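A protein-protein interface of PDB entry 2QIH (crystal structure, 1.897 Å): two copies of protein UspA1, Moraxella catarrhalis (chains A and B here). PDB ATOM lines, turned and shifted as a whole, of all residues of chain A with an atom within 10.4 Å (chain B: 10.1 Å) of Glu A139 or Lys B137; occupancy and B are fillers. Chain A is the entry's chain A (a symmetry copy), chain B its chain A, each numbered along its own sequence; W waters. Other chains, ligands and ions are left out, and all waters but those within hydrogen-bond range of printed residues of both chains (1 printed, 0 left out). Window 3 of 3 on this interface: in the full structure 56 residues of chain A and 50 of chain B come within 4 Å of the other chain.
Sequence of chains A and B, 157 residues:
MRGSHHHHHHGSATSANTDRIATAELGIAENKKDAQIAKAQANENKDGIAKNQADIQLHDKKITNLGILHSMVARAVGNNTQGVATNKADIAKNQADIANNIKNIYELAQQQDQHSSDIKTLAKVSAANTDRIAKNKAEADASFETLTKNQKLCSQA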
ATOM      1  N   ASP A 131      32.119 -33.088 -10.196  1.00  0.00           N
ATOM      2  CA  ASP A 131      32.321 -31.643 -10.328  1.00  0.00           C
ATOM      3  C   ASP A 131      31.667 -30.842  -9.182  1.00  0.00           C
ATOM      4  O   ASP A 131      32.322 -30.056  -8.523  1.00  0.00           O
ATOM      5  CB  ASP A 131      31.779 -31.165 -11.671  1.00  0.00           C
ATOM      6  CG  ASP A 131      32.210 -29.746 -12.028  1.00  0.00           C
ATOM      7  OD1 ASP A 131      31.825 -28.767 -11.330  1.00  0.00           O
ATOM      8  OD2 ASP A 131      32.900 -29.588 -13.064  1.00  0.00           O
ATOM      9  N   ARG A 132      30.376 -31.049  -8.966  1.00  0.00           N
ATOM     10  CA  ARG A 132      29.656 -30.282  -7.980  1.00  0.00           C
ATOM     11  C   ARG A 132      30.175 -30.503  -6.543  1.00  0.00           C
ATOM     12  O   ARG A 132      30.212 -29.560  -5.741  1.00  0.00           O
ATOM     13  CB  ARG A 132      28.172 -30.611  -8.015  1.00  0.00           C
ATOM     14  CG  ARG A 132      27.356 -29.550  -7.321  1.00  0.00           C
ATOM     15  CD  ARG A 132      26.737 -28.715  -8.383  1.00  0.00           C
ATOM     16  NE  ARG A 132      26.823 -27.297  -8.140  1.00  0.00           N
ATOM     17  CZ  ARG A 132      26.497 -26.374  -9.043  1.00  0.00           C
ATOM     18  NH1 ARG A 132      26.049 -26.753 -10.242  1.00  0.00           N
ATOM     19  NH2 ARG A 132      26.608 -25.081  -8.743  1.00  0.00           N
ATOM     20  N   ILE A 133      30.521 -31.740  -6.221  1.00  0.00           N
ATOM     21  CA  ILE A 133      31.094 -32.080  -4.897  1.00  0.00           C
ATOM     22  C   ILE A 133      32.326 -31.199  -4.655  1.00  0.00           C
ATOM     23  O   ILE A 133      32.468 -30.582  -3.612  1.00  0.00           O
ATOM     24  CB  ILE A 133      31.508 -33.598  -4.838  1.00  0.00           C
ATOM     25  CG1 ILE A 133      30.263 -34.516  -4.861  1.00  0.00           C
ATOM     26  CG2 ILE A 133      32.405 -33.915  -3.618  1.00  0.00           C
ATOM     27  CD1 ILE A 133      30.626 -35.966  -5.233  1.00  0.00           C
ATOM     28  N   ALA A 134      33.187 -31.110  -5.654  1.00  0.00           N
ATOM     29  CA  ALA A 134      34.453 -30.385  -5.511  1.00  0.00           C
ATOM     30  C   ALA A 134      34.215 -28.869  -5.439  1.00  0.00           C
ATOM     31  O   ALA A 134      34.883 -28.154  -4.682  1.00  0.00           O
ATOM     32  CB  ALA A 134      35.349 -30.726  -6.686  1.00  0.00           C
ATOM     33  N   LYS A 135      33.290 -28.384  -6.261  1.00  0.00           N
ATOM     34  CA  LYS A 135      32.910 -26.975  -6.276  1.00  0.00           C
ATOM     35  C   LYS A 135      32.333 -26.613  -4.923  1.00  0.00           C
ATOM     36  O   LYS A 135      32.728 -25.594  -4.347  1.00  0.00           O
ATOM     37  CB  LYS A 135      31.865 -26.696  -7.359  1.00  0.00           C
ATOM     38  CG  LYS A 135      31.466 -25.202  -7.510  1.00  0.00           C
ATOM     39  CD  LYS A 135      30.337 -25.038  -8.507  1.00  0.00           C
ATOM     40  CE  LYS A 135      30.107 -23.568  -8.792  1.00  0.00           C
ATOM     41  NZ  LYS A 135      29.178 -23.363  -9.932  1.00  0.00           N
ATOM     42  N   ASN A 136      31.355 -27.400  -4.453  1.00  0.00           N
ATOM     43  CA  ASN A 136      30.736 -27.127  -3.142  1.00  0.00           C
ATOM     44  C   ASN A 136      31.735 -27.161  -1.997  1.00  0.00           C
ATOM     45  O   ASN A 136      31.652 -26.326  -1.088  1.00  0.00           O
ATOM     46  CB  ASN A 136      29.518 -28.038  -2.884  1.00  0.00           C
ATOM     47  CG  ASN A 136      28.343 -27.717  -3.815  1.00  0.00           C
ATOM     48  OD1 ASN A 136      28.388 -26.717  -4.556  1.00  0.00           O
ATOM     49  ND2 ASN A 136      27.281 -28.554  -3.780  1.00  0.00           N
ATOM     50  N   LYS A 137      32.666 -28.117  -2.026  1.00  0.00           N
ATOM     51  CA  LYS A 137      33.747 -28.163  -1.020  1.00  0.00           C
ATOM     52  C   LYS A 137      34.551 -26.855  -1.012  1.00  0.00           C
ATOM     53  O   LYS A 137      34.810 -26.277   0.075  1.00  0.00           O
ATOM     54  CB  LYS A 137      34.657 -29.372  -1.262  1.00  0.00           C
ATOM     55  CG  LYS A 137      35.761 -29.573  -0.209  1.00  0.00           C
ATOM     56  CD  LYS A 137      35.248 -29.690   1.203  1.00  0.00           C
ATOM     57  CE  LYS A 137      36.306 -30.318   2.119  1.00  0.00           C
ATOM     58  NZ  LYS A 137      37.343 -29.352   2.591  1.00  0.00           N
ATOM     59  N   ALA A 138      34.939 -26.361  -2.199  1.00  0.00           N
ATOM     60  CA  ALA A 138      35.749 -25.122  -2.231  1.00  0.00           C
ATOM     61  C   ALA A 138      34.949 -23.937  -1.699  1.00  0.00           C
ATOM     62  O   ALA A 138      35.469 -23.172  -0.880  1.00  0.00           O
ATOM     63  CB  ALA A 138      36.320 -24.819  -3.610  1.00  0.00           C
ATOM     64  N   GLU A 139      33.686 -23.813  -2.114  1.00  0.00           N
ATOM     65  CA  GLU A 139      32.832 -22.745  -1.589  1.00  0.00           C
ATOM     66  C   GLU A 139      32.691 -22.846  -0.056  1.00  0.00           C
ATOM     67  O   GLU A 139      32.792 -21.832   0.642  1.00  0.00           O
ATOM     68  CB  GLU A 139      31.444 -22.708  -2.254  1.00  0.00           C
ATOM     69  CG  GLU A 139      31.464 -22.458  -3.762  1.00  0.00           C
ATOM     70  CD  GLU A 139      30.077 -22.576  -4.407  1.00  0.00           C
ATOM     71  OE1 GLU A 139      29.070 -22.857  -3.689  1.00  0.00           O
ATOM     72  OE2 GLU A 139      30.001 -22.398  -5.647  1.00  0.00           O
ATOM     73  N   ALA A 140      32.481 -24.041   0.474  1.00  0.00           N
ATOM     74  CA  ALA A 140      32.418 -24.191   1.949  1.00  0.00           C
ATOM     75  C   ALA A 140      33.733 -23.787   2.654  1.00  0.00           C
ATOM     76  O   ALA A 140      33.730 -23.011   3.627  1.00  0.00           O
ATOM     77  CB  ALA A 140      31.993 -25.621   2.330  1.00  0.00           C
ATOM     78  N   ASP A 141      34.855 -24.313   2.159  1.00  0.00           N
ATOM     79  CA  ASP A 141      36.156 -23.971   2.720  1.00  0.00           C
ATOM     80  C   ASP A 141      36.419 -22.449   2.693  1.00  0.00           C
ATOM     81  O   ASP A 141      36.808 -21.863   3.704  1.00  0.00           O
ATOM     82  CB  ASP A 141      37.259 -24.697   1.966  1.00  0.00           C
ATOM     83  CG  ASP A 141      37.257 -26.204   2.217  1.00  0.00           C
ATOM     84  OD1 ASP A 141      36.514 -26.728   3.113  1.00  0.00           O
ATOM     85  OD2 ASP A 141      37.975 -26.877   1.458  1.00  0.00           O
ATOM     86  N   ALA A 142      36.227 -21.816   1.542  1.00  0.00           N
ATOM     87  CA  ALA A 142      36.375 -20.365   1.461  1.00  0.00           C
ATOM     88  C   ALA A 142      35.474 -19.621   2.473  1.00  0.00           C
ATOM     89  O   ALA A 142      35.918 -18.666   3.137  1.00  0.00           O
ATOM     90  CB  ALA A 142      36.138 -19.877  -0.022  1.00  0.00           C
ATOM     91  N   SER A 143      34.234 -20.081   2.641  1.00  0.00           N
ATOM     92  CA  SER A 143      33.307 -19.431   3.600  1.00  0.00           C
ATOM     93  C   SER A 143      33.689 -19.659   5.061  1.00  0.00           C
ATOM     94  O   SER A 143      33.582 -18.740   5.886  1.00  0.00           O
ATOM     95  CB  SER A 143      31.837 -19.839   3.329  1.00  0.00           C
ATOM     96  OG  SER A 143      31.445 -19.448   2.003  1.00  0.00           O
ATOM     97  N   PHE A 144      34.114 -20.875   5.401  1.00  0.00           N
ATOM     98  CA  PHE A 144      34.683 -21.116   6.728  1.00  0.00           C
ATOM     99  C   PHE A 144      35.902 -20.257   6.966  1.00  0.00           C
ATOM    100  O   PHE A 144      36.086 -19.795   8.083  1.00  0.00           O
ATOM    101  CB  PHE A 144      35.115 -22.570   6.925  1.00  0.00           C
ATOM    102  CG  PHE A 144      33.993 -23.510   7.131  1.00  0.00           C
ATOM    103  CD1 PHE A 144      33.858 -24.623   6.324  1.00  0.00           C
ATOM    104  CD2 PHE A 144      33.078 -23.308   8.155  1.00  0.00           C
ATOM    105  CE1 PHE A 144      32.823 -25.530   6.516  1.00  0.00           C
ATOM    106  CE2 PHE A 144      32.045 -24.222   8.352  1.00  0.00           C
ATOM    107  CZ  PHE A 144      31.923 -25.333   7.513  1.00  0.00           C
ATOM    108  N   GLU A 145      36.738 -20.059   5.935  1.00  0.00           N
ATOM    109  CA  GLU A 145      37.941 -19.225   6.114  1.00  0.00           C
ATOM    110  C   GLU A 145      37.597 -17.778   6.535  1.00  0.00           C
ATOM    111  O   GLU A 145      38.231 -17.217   7.439  1.00  0.00           O
ATOM    112  CB  GLU A 145      38.864 -19.258   4.893  1.00  0.00           C
ATOM    113  CG  GLU A 145      39.963 -18.196   4.935  1.00  0.00           C
ATOM    114  CD  GLU A 145      41.290 -18.696   4.374  1.00  0.00           C
ATOM    115  OE1 GLU A 145      41.285 -19.560   3.468  1.00  0.00           O
ATOM    116  OE2 GLU A 145      42.348 -18.226   4.846  1.00  0.00           O
ATOM    117  N   THR A 146      36.581 -17.197   5.919  1.00  0.00           N
ATOM    118  CA  THR A 146      36.195 -15.829   6.242  1.00  0.00           C
ATOM    119  C   THR A 146      35.716 -15.702   7.692  1.00  0.00           C
ATOM    120  O   THR A 146      36.144 -14.779   8.415  1.00  0.00           O
ATOM    121  CB  THR A 146      35.130 -15.287   5.250  1.00  0.00           C
ATOM    122  OG1 THR A 146      33.941 -16.069   5.337  1.00  0.00           O
ATOM    123  CG2 THR A 146      35.636 -15.369   3.827  1.00  0.00           C
ATOM    124  N   LEU A 147      34.842 -16.624   8.103  1.00  0.00           N
ATOM    125  CA  LEU A 147      34.251 -16.638   9.438  1.00  0.00           C
ATOM    126  C   LEU A 147      35.290 -16.921  10.495  1.00  0.00           C
ATOM    127  O   LEU A 147      35.276 -16.304  11.554  1.00  0.00           O
ATOM    128  CB  LEU A 147      33.132 -17.692   9.544  1.00  0.00           C
ATOM    129  CG  LEU A 147      31.815 -17.462   8.793  1.00  0.00           C
ATOM    130  CD1 LEU A 147      31.014 -18.753   8.745  1.00  0.00           C
ATOM    131  CD2 LEU A 147      31.033 -16.367   9.480  1.00  0.00           C
ATOM    132  N   ASN B 129      23.271 -39.690  -4.905  1.00  0.00           N
ATOM    133  CA  ASN B 129      24.389 -38.755  -4.731  1.00  0.00           C
ATOM    134  C   ASN B 129      24.014 -37.349  -5.140  1.00  0.00           C
ATOM    135  O   ASN B 129      24.267 -36.380  -4.394  1.00  0.00           O
ATOM    136  CB  ASN B 129      25.628 -39.208  -5.518  1.00  0.00           C
ATOM    137  CG  ASN B 129      26.291 -40.426  -4.914  1.00  0.00           C
ATOM    138  OD1 ASN B 129      26.084 -40.762  -3.746  1.00  0.00           O
ATOM    139  ND2 ASN B 129      27.113 -41.078  -5.701  1.00  0.00           N
ATOM    140  N   THR B 130      23.369 -37.235  -6.301  1.00  0.00           N
ATOM    141  CA  THR B 130      22.872 -35.955  -6.771  1.00  0.00           C
ATOM    142  C   THR B 130      21.973 -35.319  -5.714  1.00  0.00           C
ATOM    143  O   THR B 130      22.191 -34.180  -5.343  1.00  0.00           O
ATOM    144  CB  THR B 130      22.031 -36.088  -8.052  1.00  0.00           C
ATOM    145  OG1 THR B 130      22.839 -36.616  -9.089  1.00  0.00           O
ATOM    146  CG2 THR B 130      21.462 -34.707  -8.461  1.00  0.00           C
ATOM    147  N   ASP B 131      20.993 -36.074  -5.223  1.00  0.00           N
ATOM    148  CA  ASP B 131      20.117 -35.621  -4.140  1.00  0.00           C
ATOM    149  C   ASP B 131      20.900 -35.141  -2.899  1.00  0.00           C
ATOM    150  O   ASP B 131      20.702 -34.035  -2.431  1.00  0.00           O
ATOM    151  CB  ASP B 131      19.159 -36.740  -3.748  1.00  0.00           C
ATOM    152  CG  ASP B 131      18.018 -36.274  -2.848  1.00  0.00           C
ATOM    153  OD1 ASP B 131      18.257 -35.839  -1.688  1.00  0.00           O
ATOM    154  OD2 ASP B 131      16.846 -36.398  -3.278  1.00  0.00           O
ATOM    155  N   ARG B 132      21.778 -35.987  -2.379  1.00  0.00           N
ATOM    156  CA  ARG B 132      22.490 -35.665  -1.169  1.00  0.00           C
ATOM    157  C   ARG B 132      23.409 -34.432  -1.314  1.00  0.00           C
ATOM    158  O   ARG B 132      23.539 -33.637  -0.374  1.00  0.00           O
ATOM    159  CB  ARG B 132      23.332 -36.844  -0.706  1.00  0.00           C
ATOM    160  CG  ARG B 132      23.737 -36.698   0.740  1.00  0.00           C
ATOM    161  CD  ARG B 132      22.855 -37.597   1.529  1.00  0.00           C
ATOM    162  NE  ARG B 132      22.323 -36.994   2.726  1.00  0.00           N
ATOM    163  CZ  ARG B 132      21.377 -37.557   3.476  1.00  0.00           C
ATOM    164  NH1 ARG B 132      20.885 -38.749   3.133  1.00  0.00           N
ATOM    165  NH2 ARG B 132      20.935 -36.933   4.567  1.00  0.00           N
ATOM    166  N   ILE B 133      24.063 -34.313  -2.458  1.00  0.00           N
ATOM    167  CA  ILE B 133      24.928 -33.147  -2.755  1.00  0.00           C
ATOM    168  C   ILE B 133      24.099 -31.866  -2.585  1.00  0.00           C
ATOM    169  O   ILE B 133      24.512 -30.930  -1.920  1.00  0.00           O
ATOM    170  CB  ILE B 133      25.489 -33.222  -4.224  1.00  0.00           C
ATOM    171  CG1 ILE B 133      26.503 -34.381  -4.374  1.00  0.00           C
ATOM    172  CG2 ILE B 133      26.110 -31.883  -4.686  1.00  0.00           C
ATOM    173  CD1 ILE B 133      26.738 -34.752  -5.850  1.00  0.00           C
ATOM    174  N   ALA B 134      22.905 -31.862  -3.151  1.00  0.00           N
ATOM    175  CA  ALA B 134      22.061 -30.664  -3.150  1.00  0.00           C
ATOM    176  C   ALA B 134      21.513 -30.377  -1.743  1.00  0.00           C
ATOM    177  O   ALA B 134      21.415 -29.220  -1.321  1.00  0.00           O
ATOM    178  CB  ALA B 134      20.923 -30.864  -4.131  1.00  0.00           C
ATOM    179  N   LYS B 135      21.120 -31.438  -1.043  1.00  0.00           N
ATOM    180  CA  LYS B 135      20.627 -31.339   0.327  1.00  0.00           C
ATOM    181  C   LYS B 135      21.734 -30.789   1.203  1.00  0.00           C
ATOM    182  O   LYS B 135      21.490 -29.860   1.980  1.00  0.00           O
ATOM    183  CB  LYS B 135      20.197 -32.707   0.860  1.00  0.00           C
ATOM    184  CG  LYS B 135      19.572 -32.685   2.282  1.00  0.00           C
ATOM    185  CD  LYS B 135      19.299 -34.090   2.779  1.00  0.00           C
ATOM    186  CE  LYS B 135      18.506 -34.039   4.068  1.00  0.00           C
ATOM    187  NZ  LYS B 135      18.011 -35.382   4.469  1.00  0.00           N
ATOM    188  N   ASN B 136      22.923 -31.405   1.132  1.00  0.00           N
ATOM    189  CA  ASN B 136      24.060 -30.937   1.947  1.00  0.00           C
ATOM    190  C   ASN B 136      24.443 -29.495   1.656  1.00  0.00           C
ATOM    191  O   ASN B 136      24.762 -28.746   2.587  1.00  0.00           O
ATOM    192  CB  ASN B 136      25.266 -31.894   1.849  1.00  0.00           C
ATOM    193  CG  ASN B 136      24.990 -33.248   2.514  1.00  0.00           C
ATOM    194  OD1 ASN B 136      23.949 -33.418   3.175  1.00  0.00           O
ATOM    195  ND2 ASN B 136      25.921 -34.216   2.352  1.00  0.00           N
ATOM    196  N   LYS B 137      24.427 -29.104   0.380  1.00  0.00           N
ATOM    197  CA  LYS B 137      24.673 -27.695   0.008  1.00  0.00           C
ATOM    198  C   LYS B 137      23.675 -26.758   0.704  1.00  0.00           C
ATOM    199  O   LYS B 137      24.082 -25.719   1.285  1.00  0.00           O
ATOM    200  CB  LYS B 137      24.627 -27.524  -1.514  1.00  0.00           C
ATOM    201  CG  LYS B 137      24.970 -26.111  -2.017  1.00  0.00           C
ATOM    202  CD  LYS B 137      26.317 -25.607  -1.563  1.00  0.00           C
ATOM    203  CE  LYS B 137      26.781 -24.431  -2.430  1.00  0.00           C
ATOM    204  NZ  LYS B 137      26.177 -23.122  -2.042  1.00  0.00           N
ATOM    205  N   ALA B 138      22.379 -27.104   0.675  1.00  0.00           N
ATOM    206  CA  ALA B 138      21.381 -26.207   1.301  1.00  0.00           C
ATOM    207  C   ALA B 138      21.599 -26.120   2.807  1.00  0.00           C
ATOM    208  O   ALA B 138      21.595 -25.014   3.359  1.00  0.00           O
ATOM    209  CB  ALA B 138      19.943 -26.595   0.979  1.00  0.00           C
ATOM    210  N   GLU B 139      21.840 -27.259   3.460  1.00  0.00           N
ATOM    211  CA  GLU B 139      22.135 -27.247   4.894  1.00  0.00           C
ATOM    212  C   GLU B 139      23.384 -26.395   5.201  1.00  0.00           C
ATOM    213  O   GLU B 139      23.374 -25.601   6.147  1.00  0.00           O
ATOM    214  CB  GLU B 139      22.293 -28.661   5.483  1.00  0.00           C
ATOM    215  CG  GLU B 139      21.050 -29.544   5.368  1.00  0.00           C
ATOM    216  CD  GLU B 139      21.294 -30.986   5.832  1.00  0.00           C
ATOM    217  OE1 GLU B 139      22.441 -31.326   6.252  1.00  0.00           O
ATOM    218  OE2 GLU B 139      20.330 -31.785   5.760  1.00  0.00           O
ATOM    219  N   ALA B 140      24.440 -26.531   4.415  1.00  0.00           N
ATOM    220  CA  ALA B 140      25.632 -25.673   4.629  1.00  0.00           C
ATOM    221  C   ALA B 140      25.331 -24.167   4.454  1.00  0.00           C
ATOM    222  O   ALA B 140      25.685 -23.336   5.309  1.00  0.00           O
ATOM    223  CB  ALA B 140      26.793 -26.124   3.722  1.00  0.00           C
ATOM    224  N   ASP B 141      24.675 -23.820   3.346  1.00  0.00           N
ATOM    225  CA  ASP B 141      24.303 -22.433   3.096  1.00  0.00           C
ATOM    226  C   ASP B 141      23.439 -21.848   4.235  1.00  0.00           C
ATOM    227  O   ASP B 141      23.723 -20.762   4.742  1.00  0.00           O
ATOM    228  CB  ASP B 141      23.558 -22.319   1.775  1.00  0.00           C
ATOM    229  CG  ASP B 141      24.456 -22.569   0.564  1.00  0.00           C
ATOM    230  OD1 ASP B 141      25.722 -22.672   0.685  1.00  0.00           O
ATOM    231  OD2 ASP B 141      23.868 -22.721  -0.520  1.00  0.00           O
ATOM    232  N   ALA B 142      22.381 -22.551   4.622  1.00  0.00           N
ATOM    233  CA  ALA B 142      21.565 -22.103   5.748  1.00  0.00           C
ATOM    234  C   ALA B 142      22.396 -21.900   7.036  1.00  0.00           C
ATOM    235  O   ALA B 142      22.223 -20.898   7.753  1.00  0.00           O
ATOM    236  CB  ALA B 142      20.353 -23.090   5.967  1.00  0.00           C
ATOM    237  N   SER B 143      23.333 -22.810   7.309  1.00  0.00           N
ATOM    238  CA  SER B 143      24.180 -22.686   8.520  1.00  0.00           C
ATOM    239  C   SER B 143      25.185 -21.538   8.442  1.00  0.00           C
ATOM    240  O   SER B 143      25.412 -20.838   9.440  1.00  0.00           O
ATOM    241  CB  SER B 143      24.878 -24.027   8.860  1.00  0.00           C
ATOM    242  OG  SER B 143      23.901 -25.051   9.107  1.00  0.00           O
ATOM    243  N   PHE B 144      25.805 -21.345   7.279  1.00  0.00           N
ATOM    244  CA  PHE B 144      26.627 -20.152   7.068  1.00  0.00           C
ATOM    245  C   PHE B 144      25.812 -18.890   7.227  1.00  0.00           C
ATOM    246  O   PHE B 144      26.332 -17.918   7.755  1.00  0.00           O
ATOM    247  CB  PHE B 144      27.251 -20.110   5.673  1.00  0.00           C
ATOM    248  CG  PHE B 144      28.386 -21.040   5.491  1.00  0.00           C
ATOM    249  CD1 PHE B 144      28.379 -21.955   4.457  1.00  0.00           C
ATOM    250  CD2 PHE B 144      29.488 -20.988   6.334  1.00  0.00           C
ATOM    251  CE1 PHE B 144      29.447 -22.823   4.257  1.00  0.00           C
ATOM    252  CE2 PHE B 144      30.560 -21.852   6.128  1.00  0.00           C
ATOM    253  CZ  PHE B 144      30.523 -22.778   5.082  1.00  0.00           C
ATOM    254  N   GLU B 145      24.555 -18.896   6.757  1.00  0.00           N
ATOM    255  CA  GLU B 145      23.717 -17.690   6.890  1.00  0.00           C
ATOM    256  C   GLU B 145      23.511 -17.275   8.364  1.00  0.00           C
ATOM    257  O   GLU B 145      23.609 -16.089   8.706  1.00  0.00           O
ATOM    258  CB  GLU B 145      22.386 -17.817   6.143  1.00  0.00           C
ATOM    259  CG  GLU B 145      21.387 -16.712   6.491  1.00  0.00           C
ATOM    260  CD  GLU B 145      20.572 -16.253   5.287  1.00  0.00           C
ATOM    261  OE1 GLU B 145      20.312 -17.071   4.376  1.00  0.00           O
ATOM    262  OE2 GLU B 145      20.191 -15.062   5.248  1.00  0.00           O
HETATM  263  O   HOH W   1      27.146 -30.282  -1.518  1.00  0.00           O
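The side-chain amino group (NZ) of Lys B137 lies within salt-bridge range of the side-chain carboxylate (OE1) of Glu A139 (3.3 Å).
The backbone carbonyl oxygen (O) of Glu A139 lies within hydrogen-bond range of the side-chain hydroxyl (OG) of Ser A143 (3.1 Å). The backbone carbonyl oxygen (O) of Ser A143 is in hydrogen-bond range of the side-chain hydroxyl (OG1) of Thr A146. The side-chain amino group (NZ) of Lys B137 lies within salt-bridge range of the side-chain carboxylate (OD2) of Asp B141, 2.8 Å away.
Among the printed residues, merely in contact across the chains: Arg A132 with Ile B133 (3.7 Å), Ile A133 with Ile B133 (3.7 Å), Asn A136 with Ile B133 (3.6 Å), Asn A136 with Lys B137 (3.5 Å), Ala A140 with Phe B144 (3.5 Å), Ser A143 with Phe B144 (3.7 Å), Phe A144 with Phe B144 (3.5 Å) and Leu A147 with Phe B144 (3.6 Å).
Printed residues of chain B within 4 Å of Arg A132: Ile B133 (3.7 Å). Asn A136 touches two residues of chain B. Ala A138 touches none of the printed residues of chain B. Of chain B, only Lys B137 comes within 4 Å of Glu A139. Of chain B, only Phe B144 (3.5 Å) comes within 4 Å of Ala A140. No residue of chain B comes within 4 Å of Ala A142. Printed residues of chain B within 4 Å of Ser A143: Phe B144 (3.7 Å). Printed residues of chain B within 4 Å of Phe A144: Phe B144. Arg B132 touches none of the printed residues of chain A. Of the printed residues of chain A, Ile B133 touches Arg A132, Ile A133 and Asn A136. No residue of chain A comes within 4 Å of Ala B134. Lys B137 touches just these residues of chain A: Asn A136 and Glu A139. No residue of chain A comes within 4 Å of Ala B138. Of the printed residues of chain A, Phe B144 touches Ala A140 (3.5 Å), Ser A143 (3.7 Å), Phe A144 (3.5 Å) and Leu A147 (3.6 Å). The nearest residue of chain B that does not touch Glu A139 is Phe B144 (5.0 Å). The nearest printed residue of chain B that does not touch Ile A133 is Asn B129 (6.0 Å).
Of the 17 printed residues of chain A, 8 touch a printed residue of chain B. Printed residues of chain A that touch a printed residue of chain B: Arg A132, Ile A133, Asn A136, Glu A139, Ala A140, Ser A143, Phe A144 and Leu A147. Among the printed residues, 9 pairs touch across the chains.
Glu A139 touches Lys B137, but with the chains exchanged Lys A137 does not touch Glu B139 (11.9 Å). Ala A140 touches Phe B144, but with the chains exchanged Phe A144 does not touch Ala B140 (6.4 Å). Ser A143 touches Phe B144, but with the chains exchanged Phe A144 does not touch Ser B143 (7.2 Å). Phe A144 touches its own counterpart, Phe B144. 15 positions are printed for both chains. Of the 9 pairs that touch across the chains among the printed residues, 2 have their exchanged pair printed and touching as well.
Water W1 lies within hydrogen-bond range of the backbone carbonyl oxygen (O) of Ile B133 (2.7 Å) and the side-chain amide nitrogen (ND2) of Asn A136 (2.8 Å).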
